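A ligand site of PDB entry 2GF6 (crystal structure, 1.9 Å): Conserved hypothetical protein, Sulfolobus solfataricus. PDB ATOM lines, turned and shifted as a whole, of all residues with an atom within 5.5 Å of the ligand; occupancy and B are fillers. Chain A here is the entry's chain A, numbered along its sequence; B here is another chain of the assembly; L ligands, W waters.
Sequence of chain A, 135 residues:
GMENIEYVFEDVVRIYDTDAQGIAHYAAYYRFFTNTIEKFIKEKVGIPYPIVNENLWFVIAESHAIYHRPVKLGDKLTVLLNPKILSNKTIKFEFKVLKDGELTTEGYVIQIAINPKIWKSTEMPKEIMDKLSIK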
ATOM      1  N   VAL A  59      28.395   2.892   5.043  1.00  0.00           N
ATOM      2  CA  VAL A  59      29.490   2.153   4.428  1.00  0.00           C
ATOM      3  C   VAL A  59      28.940   1.108   3.495  1.00  0.00           C
ATOM      4  O   VAL A  59      27.956   0.449   3.838  1.00  0.00           O
ATOM      5  CB  VAL A  59      30.469   1.506   5.481  1.00  0.00           C
ATOM      6  CG1 VAL A  59      30.987   2.573   6.469  1.00  0.00           C
ATOM      7  CG2 VAL A  59      29.859   0.329   6.218  1.00  0.00           C
ATOM      8  N   ILE A  60      29.609   0.912   2.336  1.00  0.00           N
ATOM      9  CA  ILE A  60      29.199  -0.048   1.308  1.00  0.00           C
ATOM     10  C   ILE A  60      29.486  -1.498   1.729  1.00  0.00           C
ATOM     11  O   ILE A  60      30.609  -1.831   2.124  1.00  0.00           O
ATOM     12  CB  ILE A  60      29.925   0.240  -0.043  1.00  0.00           C
ATOM     13  CG1 ILE A  60      29.603   1.650  -0.534  1.00  0.00           C
ATOM     14  CG2 ILE A  60      29.569  -0.768  -1.141  1.00  0.00           C
ATOM     15  CD1 ILE A  60      30.579   2.176  -1.550  1.00  0.00           C
ATOM     16  N   ALA A  61      28.456  -2.336   1.661  1.00  0.00           N
ATOM     17  CA  ALA A  61      28.555  -3.758   1.967  1.00  0.00           C
ATOM     18  C   ALA A  61      28.647  -4.613   0.739  1.00  0.00           C
ATOM     19  O   ALA A  61      29.072  -5.765   0.807  1.00  0.00           O
ATOM     20  CB  ALA A  61      27.340  -4.149   2.729  1.00  0.00           C
ATOM     21  N   GLU A  62      28.192  -4.081  -0.395  1.00  0.00           N
ATOM     22  CA  GLU A  62      28.142  -4.905  -1.582  1.00  0.00           C
ATOM     23  C   GLU A  62      27.947  -3.994  -2.751  1.00  0.00           C
ATOM     24  O   GLU A  62      27.220  -3.011  -2.630  1.00  0.00           O
ATOM     25  CB  GLU A  62      26.961  -5.890  -1.507  1.00  0.00           C
ATOM     26  CG  GLU A  62      26.902  -6.781  -2.738  1.00  0.00           C
ATOM     27  CD  GLU A  62      25.852  -7.848  -2.680  1.00  0.00           C
ATOM     28  OE1 GLU A  62      25.297  -8.042  -1.565  1.00  0.00           O
ATOM     29  OE2 GLU A  62      25.590  -8.467  -3.772  1.00  0.00           O
ATOM     30  N   LEU A  86      15.875  -2.000   2.708  1.00  0.00           N
ATOM     31  CA  LEU A  86      15.867  -3.434   3.105  1.00  0.00           C
ATOM     32  C   LEU A  86      15.619  -3.693   4.596  1.00  0.00           C
ATOM     33  O   LEU A  86      15.114  -4.763   4.977  1.00  0.00           O
ATOM     34  CB  LEU A  86      17.193  -4.092   2.729  1.00  0.00           C
ATOM     35  CG  LEU A  86      17.680  -3.848   1.306  1.00  0.00           C
ATOM     36  CD1 LEU A  86      18.908  -4.688   1.052  1.00  0.00           C
ATOM     37  CD2 LEU A  86      16.614  -4.144   0.312  1.00  0.00           C
ATOM     38  N   SER A  87      15.952  -2.742   5.434  1.00  0.00           N
ATOM     39  CA  SER A  87      15.787  -2.902   6.862  1.00  0.00           C
ATOM     40  C   SER A  87      15.805  -1.562   7.601  1.00  0.00           C
ATOM     41  O   SER A  87      15.891  -0.492   6.981  1.00  0.00           O
ATOM     42  CB  SER A  87      16.893  -3.829   7.384  1.00  0.00           C
ATOM     43  OG  SER A  87      18.151  -3.196   7.338  1.00  0.00           O
ATOM     44  N   ASN A  88      15.773  -1.633   8.922  1.00  0.00           N
ATOM     45  CA  ASN A  88      15.997  -0.450   9.763  1.00  0.00           C
ATOM     46  C   ASN A  88      17.402   0.147   9.626  1.00  0.00           C
ATOM     47  O   ASN A  88      17.688   1.198  10.205  1.00  0.00           O
ATOM     48  CB  ASN A  88      15.621  -0.724  11.251  1.00  0.00           C
ATOM     49  CG  ASN A  88      16.556  -1.725  11.955  1.00  0.00           C
ATOM     50  OD1 ASN A  88      17.119  -2.595  11.348  1.00  0.00           O
ATOM     51  ND2 ASN A  88      16.663  -1.613  13.250  1.00  0.00           N
ATOM     52  N   LYS A  89      18.269  -0.471   8.841  1.00  0.00           N
ATOM     53  CA  LYS A  89      19.644  -0.005   8.756  1.00  0.00           C
ATOM     54  C   LYS A  89      20.373  -0.152   7.436  1.00  0.00           C
ATOM     55  O   LYS A  89      21.489   0.331   7.341  1.00  0.00           O
ATOM     56  CB  LYS A  89      20.482  -0.681   9.848  1.00  0.00           C
ATOM     57  CG  LYS A  89      20.561  -2.167   9.784  1.00  0.00           C
ATOM     58  CD  LYS A  89      21.455  -2.724  10.899  1.00  0.00           C
ATOM     59  CE  LYS A  89      20.874  -2.514  12.269  1.00  0.00           C
ATOM     60  NZ  LYS A  89      21.703  -3.233  13.324  1.00  0.00           N
ATOM     61  N   THR A  90      19.747  -0.777   6.436  1.00  0.00           N
ATOM     62  CA  THR A  90      20.383  -1.065   5.152  1.00  0.00           C
ATOM     63  C   THR A  90      19.509  -0.570   3.986  1.00  0.00           C
ATOM     64  O   THR A  90      18.279  -0.716   4.009  1.00  0.00           O
ATOM     65  CB  THR A  90      20.559  -2.556   4.999  1.00  0.00           C
ATOM     66  OG1 THR A  90      21.403  -3.038   6.048  1.00  0.00           O
ATOM     67  CG2 THR A  90      21.195  -2.844   3.715  1.00  0.00           C
ATOM     68  N   ILE A 110      24.816  -1.497  -1.925  1.00  0.00           N
ATOM     69  CA  ILE A 110      24.115  -1.666  -0.707  1.00  0.00           C
ATOM     70  C   ILE A 110      24.884  -0.971   0.392  1.00  0.00           C
ATOM     71  O   ILE A 110      26.059  -1.214   0.610  1.00  0.00           O
ATOM     72  CB  ILE A 110      23.923  -3.134  -0.448  1.00  0.00           C
ATOM     73  CG1 ILE A 110      22.935  -3.668  -1.497  1.00  0.00           C
ATOM     74  CG2 ILE A 110      23.526  -3.373   1.015  1.00  0.00           C
ATOM     75  CD1 ILE A 110      22.536  -5.061  -1.351  1.00  0.00           C
ATOM     76  N   ILE A 112      25.020   0.373   4.505  1.00  0.00           N
ATOM     77  CA  ILE A 112      24.627   0.068   5.854  1.00  0.00           C
ATOM     78  C   ILE A 112      25.019   1.243   6.724  1.00  0.00           C
ATOM     79  O   ILE A 112      26.113   1.762   6.602  1.00  0.00           O
ATOM     80  CB  ILE A 112      25.286  -1.256   6.342  1.00  0.00           C
ATOM     81  CG1 ILE A 112      24.977  -2.404   5.367  1.00  0.00           C
ATOM     82  CG2 ILE A 112      24.823  -1.645   7.733  1.00  0.00           C
ATOM     83  CD1 ILE A 112      25.651  -3.695   5.751  1.00  0.00           C
ATOM     84  N   ILE A 114      26.189   2.695  10.189  1.00  0.00           N
ATOM     85  CA  ILE A 114      27.020   2.223  11.277  1.00  0.00           C
ATOM     86  C   ILE A 114      27.384   3.281  12.299  1.00  0.00           C
ATOM     87  O   ILE A 114      27.380   4.468  11.990  1.00  0.00           O
ATOM     88  CB  ILE A 114      28.338   1.552  10.770  1.00  0.00           C
ATOM     89  CG1 ILE A 114      29.302   2.586  10.150  1.00  0.00           C
ATOM     90  CG2 ILE A 114      28.030   0.484   9.796  1.00  0.00           C
ATOM     91  CD1 ILE A 114      30.732   2.071   9.941  1.00  0.00           C
ATOM     92  N   TRP A 119      32.385   0.598  15.254  1.00  0.00           N
ATOM     93  CA  TRP A 119      32.335  -0.113  13.984  1.00  0.00           C
ATOM     94  C   TRP A 119      31.328  -1.306  13.909  1.00  0.00           C
ATOM     95  O   TRP A 119      31.641  -2.381  13.409  1.00  0.00           O
ATOM     96  CB  TRP A 119      33.759  -0.529  13.551  1.00  0.00           C
ATOM     97  CG  TRP A 119      33.833  -0.633  12.062  1.00  0.00           C
ATOM     98  CD1 TRP A 119      33.642  -1.748  11.339  1.00  0.00           C
ATOM     99  CD2 TRP A 119      34.027   0.437  11.110  1.00  0.00           C
ATOM    100  NE1 TRP A 119      33.734  -1.469   9.990  1.00  0.00           N
ATOM    101  CE2 TRP A 119      33.950  -0.128   9.830  1.00  0.00           C
ATOM    102  CE3 TRP A 119      34.264   1.813  11.220  1.00  0.00           C
ATOM    103  CZ2 TRP A 119      34.125   0.615   8.670  1.00  0.00           C
ATOM    104  CZ3 TRP A 119      34.430   2.561  10.059  1.00  0.00           C
ATOM    105  CH2 TRP A 119      34.356   1.972   8.812  1.00  0.00           C
ATOM    106  N   LYS A 120      30.108  -1.084  14.397  1.00  0.00           N
ATOM    107  CA  LYS A 120      29.005  -2.046  14.254  1.00  0.00           C
ATOM    108  C   LYS A 120      27.829  -1.304  13.624  1.00  0.00           C
ATOM    109  O   LYS A 120      27.712  -0.097  13.746  1.00  0.00           O
ATOM    110  CB  LYS A 120      28.498  -2.598  15.599  1.00  0.00           C
ATOM    111  CG  LYS A 120      29.397  -3.501  16.440  1.00  0.00           C
ATOM    112  CD  LYS A 120      30.429  -4.280  15.640  1.00  0.00           C
ATOM    113  CE  LYS A 120      31.270  -5.212  16.569  1.00  0.00           C
ATOM    114  NZ  LYS A 120      31.162  -4.911  18.052  1.00  0.00           N
ATOM    115  N   SER A 121      26.940  -2.044  12.974  1.00  0.00           N
ATOM    116  CA  SER A 121      25.843  -1.438  12.236  1.00  0.00           C
ATOM    117  C   SER A 121      24.896  -0.911  13.287  1.00  0.00           C
ATOM    118  O   SER A 121      24.970  -1.350  14.419  1.00  0.00           O
ATOM    119  CB  SER A 121      25.183  -2.451  11.298  1.00  0.00           C
ATOM    120  OG  SER A 121      24.602  -3.529  12.006  1.00  0.00           O
ATOM    121  N   ILE B  23      39.101   3.757   5.707  1.00  0.00           N
ATOM    122  CA  ILE B  23      39.159   2.406   5.231  1.00  0.00           C
ATOM    123  C   ILE B  23      39.415   2.483   3.742  1.00  0.00           C
ATOM    124  O   ILE B  23      39.234   3.542   3.124  1.00  0.00           O
ATOM    125  CB  ILE B  23      37.808   1.663   5.492  1.00  0.00           C
ATOM    126  CG1 ILE B  23      36.657   2.299   4.694  1.00  0.00           C
ATOM    127  CG2 ILE B  23      37.488   1.672   6.974  1.00  0.00           C
ATOM    128  CD1 ILE B  23      35.336   1.631   4.909  1.00  0.00           C
ATOM    129  N   ALA B  24      39.828   1.356   3.167  1.00  0.00           N
ATOM    130  CA  ALA B  24      40.048   1.293   1.731  1.00  0.00           C
ATOM    131  C   ALA B  24      38.752   1.576   1.009  1.00  0.00           C
ATOM    132  O   ALA B  24      37.691   1.168   1.445  1.00  0.00           O
ATOM    133  CB  ALA B  24      40.584  -0.043   1.346  1.00  0.00           C
ATOM    134  N   HIS B  25      38.859   2.256  -0.121  1.00  0.00           N
ATOM    135  CA  HIS B  25      37.722   2.673  -0.882  1.00  0.00           C
ATOM    136  C   HIS B  25      37.478   1.790  -2.113  1.00  0.00           C
ATOM    137  O   HIS B  25      38.279   0.939  -2.464  1.00  0.00           O
ATOM    138  CB  HIS B  25      37.866   4.153  -1.289  1.00  0.00           C
ATOM    139  CG  HIS B  25      39.135   4.489  -2.008  1.00  0.00           C
ATOM    140  ND1 HIS B  25      39.578   3.799  -3.115  1.00  0.00           N
ATOM    141  CD2 HIS B  25      40.016   5.506  -1.826  1.00  0.00           C
ATOM    142  CE1 HIS B  25      40.711   4.327  -3.548  1.00  0.00           C
ATOM    143  NE2 HIS B  25      40.981   5.383  -2.799  1.00  0.00           N
ATOM    144  N   TYR B  26      36.349   2.020  -2.760  1.00  0.00           N
ATOM    145  CA  TYR B  26      35.865   1.220  -3.886  1.00  0.00           C
ATOM    146  C   TYR B  26      36.940   1.000  -4.947  1.00  0.00           C
ATOM    147  O   TYR B  26      37.071  -0.093  -5.485  1.00  0.00           O
ATOM    148  CB  TYR B  26      34.641   1.934  -4.477  1.00  0.00           C
ATOM    149  CG  TYR B  26      33.895   1.257  -5.646  1.00  0.00           C
ATOM    150  CD1 TYR B  26      32.898   0.307  -5.414  1.00  0.00           C
ATOM    151  CD2 TYR B  26      34.165   1.605  -6.953  1.00  0.00           C
ATOM    152  CE1 TYR B  26      32.227  -0.305  -6.450  1.00  0.00           C
ATOM    153  CE2 TYR B  26      33.486   1.009  -8.022  1.00  0.00           C
ATOM    154  CZ  TYR B  26      32.541   0.051  -7.783  1.00  0.00           C
ATOM    155  OH  TYR B  26      31.864  -0.523  -8.855  1.00  0.00           O
ATOM    156  N   TYR B  29      40.014  -1.486  -4.303  1.00  0.00           N
ATOM    157  CA  TYR B  29      39.855  -2.938  -4.507  1.00  0.00           C
ATOM    158  C   TYR B  29      40.134  -3.295  -5.945  1.00  0.00           C
ATOM    159  O   TYR B  29      40.659  -4.349  -6.241  1.00  0.00           O
ATOM    160  CB  TYR B  29      38.471  -3.427  -4.057  1.00  0.00           C
ATOM    161  CG  TYR B  29      38.320  -3.404  -2.547  1.00  0.00           C
ATOM    162  CD1 TYR B  29      38.777  -4.449  -1.779  1.00  0.00           C
ATOM    163  CD2 TYR B  29      37.748  -2.339  -1.892  1.00  0.00           C
ATOM    164  CE1 TYR B  29      38.669  -4.445  -0.374  1.00  0.00           C
ATOM    165  CE2 TYR B  29      37.617  -2.333  -0.490  1.00  0.00           C
ATOM    166  CZ  TYR B  29      38.078  -3.382   0.249  1.00  0.00           C
ATOM    167  OH  TYR B  29      37.976  -3.395   1.626  1.00  0.00           O
ATOM    168  N   ILE B  66      31.467  -8.132  -2.404  1.00  0.00           N
ATOM    169  CA  ILE B  66      30.806  -8.194  -1.113  1.00  0.00           C
ATOM    170  C   ILE B  66      31.906  -7.860  -0.108  1.00  0.00           C
ATOM    171  O   ILE B  66      32.911  -8.546  -0.050  1.00  0.00           O
ATOM    172  CB  ILE B  66      30.268  -9.634  -0.814  1.00  0.00           C
ATOM    173  CG1 ILE B  66      29.145 -10.010  -1.765  1.00  0.00           C
ATOM    174  CG2 ILE B  66      29.782  -9.738   0.613  1.00  0.00           C
ATOM    175  CD1 ILE B  66      28.711 -11.441  -1.618  1.00  0.00           C
ATOM    176  N   TYR B  67      31.738  -6.780   0.650  1.00  0.00           N
ATOM    177  CA  TYR B  67      32.805  -6.303   1.533  1.00  0.00           C
ATOM    178  C   TYR B  67      32.508  -6.699   2.963  1.00  0.00           C
ATOM    179  O   TYR B  67      31.754  -6.002   3.651  1.00  0.00           O
ATOM    180  CB  TYR B  67      32.952  -4.777   1.394  1.00  0.00           C
ATOM    181  CG  TYR B  67      32.986  -4.290  -0.046  1.00  0.00           C
ATOM    182  CD1 TYR B  67      31.814  -3.965  -0.728  1.00  0.00           C
ATOM    183  CD2 TYR B  67      34.189  -4.171  -0.737  1.00  0.00           C
ATOM    184  CE1 TYR B  67      31.864  -3.518  -2.060  1.00  0.00           C
ATOM    185  CE2 TYR B  67      34.233  -3.731  -2.059  1.00  0.00           C
ATOM    186  CZ  TYR B  67      33.072  -3.399  -2.711  1.00  0.00           C
ATOM    187  OH  TYR B  67      33.124  -2.964  -4.031  1.00  0.00           O
ATOM    188  N   HIS B  68      33.059  -7.815   3.436  1.00  0.00           N
ATOM    189  CA  HIS B  68      32.615  -8.398   4.720  1.00  0.00           C
ATOM    190  C   HIS B  68      33.214  -7.655   5.875  1.00  0.00           C
ATOM    191  O   HIS B  68      32.597  -7.519   6.936  1.00  0.00           O
ATOM    192  CB  HIS B  68      33.054  -9.848   4.884  1.00  0.00           C
ATOM    193  CG  HIS B  68      32.601 -10.761   3.795  1.00  0.00           C
ATOM    194  ND1 HIS B  68      31.327 -11.294   3.747  1.00  0.00           N
ATOM    195  CD2 HIS B  68      33.272 -11.294   2.746  1.00  0.00           C
ATOM    196  CE1 HIS B  68      31.231 -12.096   2.694  1.00  0.00           C
ATOM    197  NE2 HIS B  68      32.396 -12.114   2.075  1.00  0.00           N
ATOM    198  N   ARG B  69      34.457  -7.242   5.691  1.00  0.00           N
ATOM    199  CA  ARG B  69      35.212  -6.623   6.746  1.00  0.00           C
ATOM    200  C   ARG B  69      36.025  -5.459   6.155  1.00  0.00           C
ATOM    201  O   ARG B  69      36.348  -5.431   4.982  1.00  0.00           O
ATOM    202  CB  ARG B  69      36.100  -7.667   7.430  1.00  0.00           C
ATOM    203  CG  ARG B  69      35.355  -8.963   7.851  1.00  0.00           C
ATOM    204  CD  ARG B  69      36.278  -9.998   8.436  1.00  0.00           C
ATOM    205  NE  ARG B  69      36.946  -9.494   9.647  1.00  0.00           N
ATOM    206  CZ  ARG B  69      37.851 -10.171  10.361  1.00  0.00           C
ATOM    207  NH1 ARG B  69      38.187 -11.427  10.046  1.00  0.00           N
ATOM    208  NH2 ARG B  69      38.402  -9.614  11.421  1.00  0.00           N
ATOM    209  N   PRO B  70      36.324  -4.452   6.973  1.00  0.00           N
ATOM    210  CA  PRO B  70      37.047  -3.301   6.445  1.00  0.00           C
ATOM    211  C   PRO B  70      38.558  -3.610   6.414  1.00  0.00           C
ATOM    212  O   PRO B  70      39.029  -4.426   7.228  1.00  0.00           O
ATOM    213  CB  PRO B  70      36.722  -2.195   7.446  1.00  0.00           C
ATOM    214  CG  PRO B  70      36.662  -2.954   8.772  1.00  0.00           C
ATOM    215  CD  PRO B  70      36.070  -4.322   8.429  1.00  0.00           C
ATOM    216  N   VAL B  71      39.278  -3.016   5.473  1.00  0.00           N
ATOM    217  CA  VAL B  71      40.741  -2.976   5.508  1.00  0.00           C
ATOM    218  C   VAL B  71      41.213  -1.518   5.696  1.00  0.00           C
ATOM    219  O   VAL B  71      40.668  -0.612   5.076  1.00  0.00           O
ATOM    220  CB  VAL B  71      41.382  -3.629   4.276  1.00  0.00           C
ATOM    221  CG1 VAL B  71      40.919  -5.068   4.097  1.00  0.00           C
ATOM    222  CG2 VAL B  71      41.087  -2.882   3.044  1.00  0.00           C
HETATM  223  N1  LIG L   1      22.853  -7.050   1.485  1.00  0.00           N
HETATM  224  C1  LIG L   1      21.767  -6.870   2.337  1.00  0.00           C
HETATM  225  N2  LIG L   1      21.963  -6.844   3.702  1.00  0.00           N
HETATM  226  C2  LIG L   1      23.212  -7.004   4.182  1.00  0.00           C
HETATM  227  C3  LIG L   1      24.300  -7.196   3.342  1.00  0.00           C
HETATM  228  C4  LIG L   1      24.123  -7.210   1.977  1.00  0.00           C
HETATM  229  N3  LIG L   1      25.141  -7.615   1.204  1.00  0.00           N
HETATM  230  N4  LIG L   1      25.407  -7.314   4.095  1.00  0.00           N
HETATM  231  C5  LIG L   1      25.057  -7.189   5.409  1.00  0.00           C
HETATM  232  N5  LIG L   1      23.697  -7.019   5.452  1.00  0.00           N
HETATM  233  C6  LIG L   1      22.814  -6.996   6.618  1.00  0.00           C
HETATM  234  C7  LIG L   1      22.914  -8.202   7.517  1.00  0.00           C
HETATM  235  O1  LIG L   1      22.133  -9.270   7.068  1.00  0.00           O
HETATM  236  C8  LIG L   1      22.358  -7.646   8.800  1.00  0.00           C
HETATM  237  O2  LIG L   1      20.943  -7.778   8.720  1.00  0.00           O
HETATM  238  P1  LIG L   1      19.946  -7.832   9.993  1.00  0.00           P
HETATM  239  O3  LIG L   1      19.206  -6.504  10.043  1.00  0.00           O
HETATM  240  O4  LIG L   1      20.666  -8.049  11.313  1.00  0.00           O
HETATM  241  O5  LIG L   1      18.943  -8.920   9.724  1.00  0.00           O
HETATM  242  C9  LIG L   1      22.774  -6.188   8.779  1.00  0.00           C
HETATM  243  O6  LIG L   1      23.145  -5.915   7.442  1.00  0.00           O
HETATM  244  C10 LIG L   1      23.948  -5.881   9.673  1.00  0.00           C
HETATM  245  O7  LIG L   1      25.040  -6.634   9.222  1.00  0.00           O
HETATM  246  P2  LIG L   1      25.975  -7.469  10.221  1.00  0.00           P
HETATM  247  O8  LIG L   1      26.522  -8.706   9.583  1.00  0.00           O
HETATM  248  O9  LIG L   1      25.297  -7.730  11.523  1.00  0.00           O
HETATM  249  O10 LIG L   1      27.222  -6.457  10.323  1.00  0.00           O
HETATM  250  P3  LIG L   1      27.808  -5.666  11.582  1.00  0.00           P
HETATM  251  O11 LIG L   1      28.653  -6.471  12.517  1.00  0.00           O
HETATM  252  O12 LIG L   1      26.817  -4.831  12.339  1.00  0.00           O
HETATM  253  O13 LIG L   1      28.784  -4.706  10.779  1.00  0.00           O
HETATM  254  C11 LIG L   1      30.106  -4.015   9.053  1.00  0.00           C
HETATM  255  C12 LIG L   1      28.725  -4.536   9.376  1.00  0.00           C
HETATM  256  C13 LIG L   1      31.107  -4.754   9.947  1.00  0.00           C
HETATM  257  C14 LIG L   1      30.106  -2.519   9.367  1.00  0.00           C
HETATM  258  C15 LIG L   1      30.455  -4.298   7.605  1.00  0.00           C
HETATM  259  O14 LIG L   1      30.490  -5.684   7.343  1.00  0.00           O
HETATM  260  C16 LIG L   1      31.781  -3.759   7.193  1.00  0.00           C
HETATM  261  O15 LIG L   1      32.633  -3.022   8.033  1.00  0.00           O
HETATM  262  N6  LIG L   1      32.088  -4.030   5.952  1.00  0.00           N
HETATM  263  C17 LIG L   1      33.210  -3.350   5.369  1.00  0.00           C
HETATM  264  C18 LIG L   1      32.681  -2.403   4.332  1.00  0.00           C
HETATM  265  C19 LIG L   1      33.799  -1.789   3.554  1.00  0.00           C
HETATM  266  O16 LIG L   1      35.001  -1.831   3.903  1.00  0.00           O
HETATM  267  N7  LIG L   1      33.341  -1.229   2.457  1.00  0.00           N
HETATM  268  C20 LIG L   1      34.255  -0.938   1.390  1.00  0.00           C
HETATM  269  C21 LIG L   1      33.482  -0.507   0.171  1.00  0.00           C
HETATM  270  S1  LIG L   1      34.652  -0.075  -1.056  1.00  0.00           S
HETATM  271  O   HOH W   1      32.431  -7.740   9.545  1.00  0.00           O
HETATM  272  O   HOH W   2      19.470  -6.476   4.854  1.00  0.00           O
HETATM  273  O   HOH W   3      22.758  -8.975  -0.937  1.00  0.00           O
HETATM  274  O   HOH W   4      24.551 -10.631   0.089  1.00  0.00           O
HETATM  275  O   HOH W   5      37.444  -1.109   3.026  1.00  0.00           O
HETATM  276  O   HOH W   6      19.796  -4.975   7.056  1.00  0.00           O
HETATM  277  O   HOH W   7      16.613  -6.971   9.385  1.00  0.00           O
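Merely in contact with the ligand: Ala 61, Leu 86, Thr 90, Ile 110, Ile 112, Ile 114, Lys 120, Ile 23 of chain B, His 25 of chain B, Tyr 29 of chain B, Arg 69 of chain B and Pro 70 of chain B. Hydrophobic or aromatic side chains within 4 Å of the ligand: Ile 60, Ala 61, Leu 86, Ile 110, Ile 112, Ile 114, Trp 119, Ile 23 of chain B, Tyr 26 of chain B, Tyr 29 of chain B, Tyr 67 of chain B and Pro 70 of chain B. 19 residues have an atom within 4 Å of the ligand: Ile 60, Ala 61, Glu 62, Leu 86, Thr 90, Ile 110, Ile 112, Ile 114, Trp 119, Lys 120, Ser 121, Ile 23 of chain B, His 25 of chain B, Tyr 26 of chain B, Tyr 29 of chain B, Tyr 67 of chain B, His 68 of chain B, Arg 69 of chain B and Pro 70 of chain B. The nearest printed residue that does not touch the ligand is Ala 24 of chain B (4.03 Å).
The backbone NH (N) of Ser 121 lies within hydrogen-bond range of an oxygen (O12) of the ligand, at 2.9 Å. The side-chain hydroxyl of Ser 121 lies within hydrogen-bond range of an oxygen (O12) of the ligand (2.6 Å). O15 of the ligand lies within hydrogen-bond range of NE1 of Trp 119, 2.7 Å away. The side-chain carboxylate of Glu 62 lies within hydrogen-bond range of a nitrogen (N3) of the ligand, at 2.8 Å. The backbone carbonyl oxygen (O) of Ile 60 sits at hydrogen-bond distance from a nitrogen (N7) of the ligand, 2.8 Å away. O14 of the ligand lies within hydrogen-bond range of O of His 68 of chain B (2.8 Å). The backbone carbonyl oxygen (O) of Tyr 67 of chain B sits at hydrogen-bond distance from a nitrogen (N6) of the ligand (3.0 Å). N of Tyr 26 of chain B sits close to S1 of the ligand (3.2 Å).
OG of Ser 121 is in hydrogen-bond range of NZ of Lys 89. The backbone NH of Ile 110 sits at hydrogen-bond distance from the backbone carbonyl oxygen of Glu 62 (2.9 Å). N of Tyr 67 of chain B lies within hydrogen-bond range of O of Ala 61 (2.9 Å). The backbone NH (N) of Ala 61 is in hydrogen-bond range of the backbone carbonyl oxygen (O) of Ile 110 (2.8 Å). N of Val 59 sits at hydrogen-bond distance from O of Ile 112, 3.0 Å away. The side-chain hydroxyl of Ser 87 sits at hydrogen-bond distance from the backbone NH of Thr 90 (3.0 Å).
Water W5 lies within hydrogen-bond range of O16 of the ligand (2.7 Å), OH of Tyr 29 of chain B (2.7 Å) and O of Ala 24 of chain B (2.8 Å). Water W3 bridges the side-chain carboxylate (OE1) of Glu 62 (2.8 Å) and a nitrogen (N1) of the ligand (3.1 Å). Water W4 lies within hydrogen-bond range of OE1 of Glu 62 (3.2 Å) and N3 of the ligand (3.3 Å). Water W6 lies within hydrogen-bond range of OG of Ser 87 (2.4 Å), OG1 of Thr 90 (2.7 Å) and O3 of the ligand (3.4 Å).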
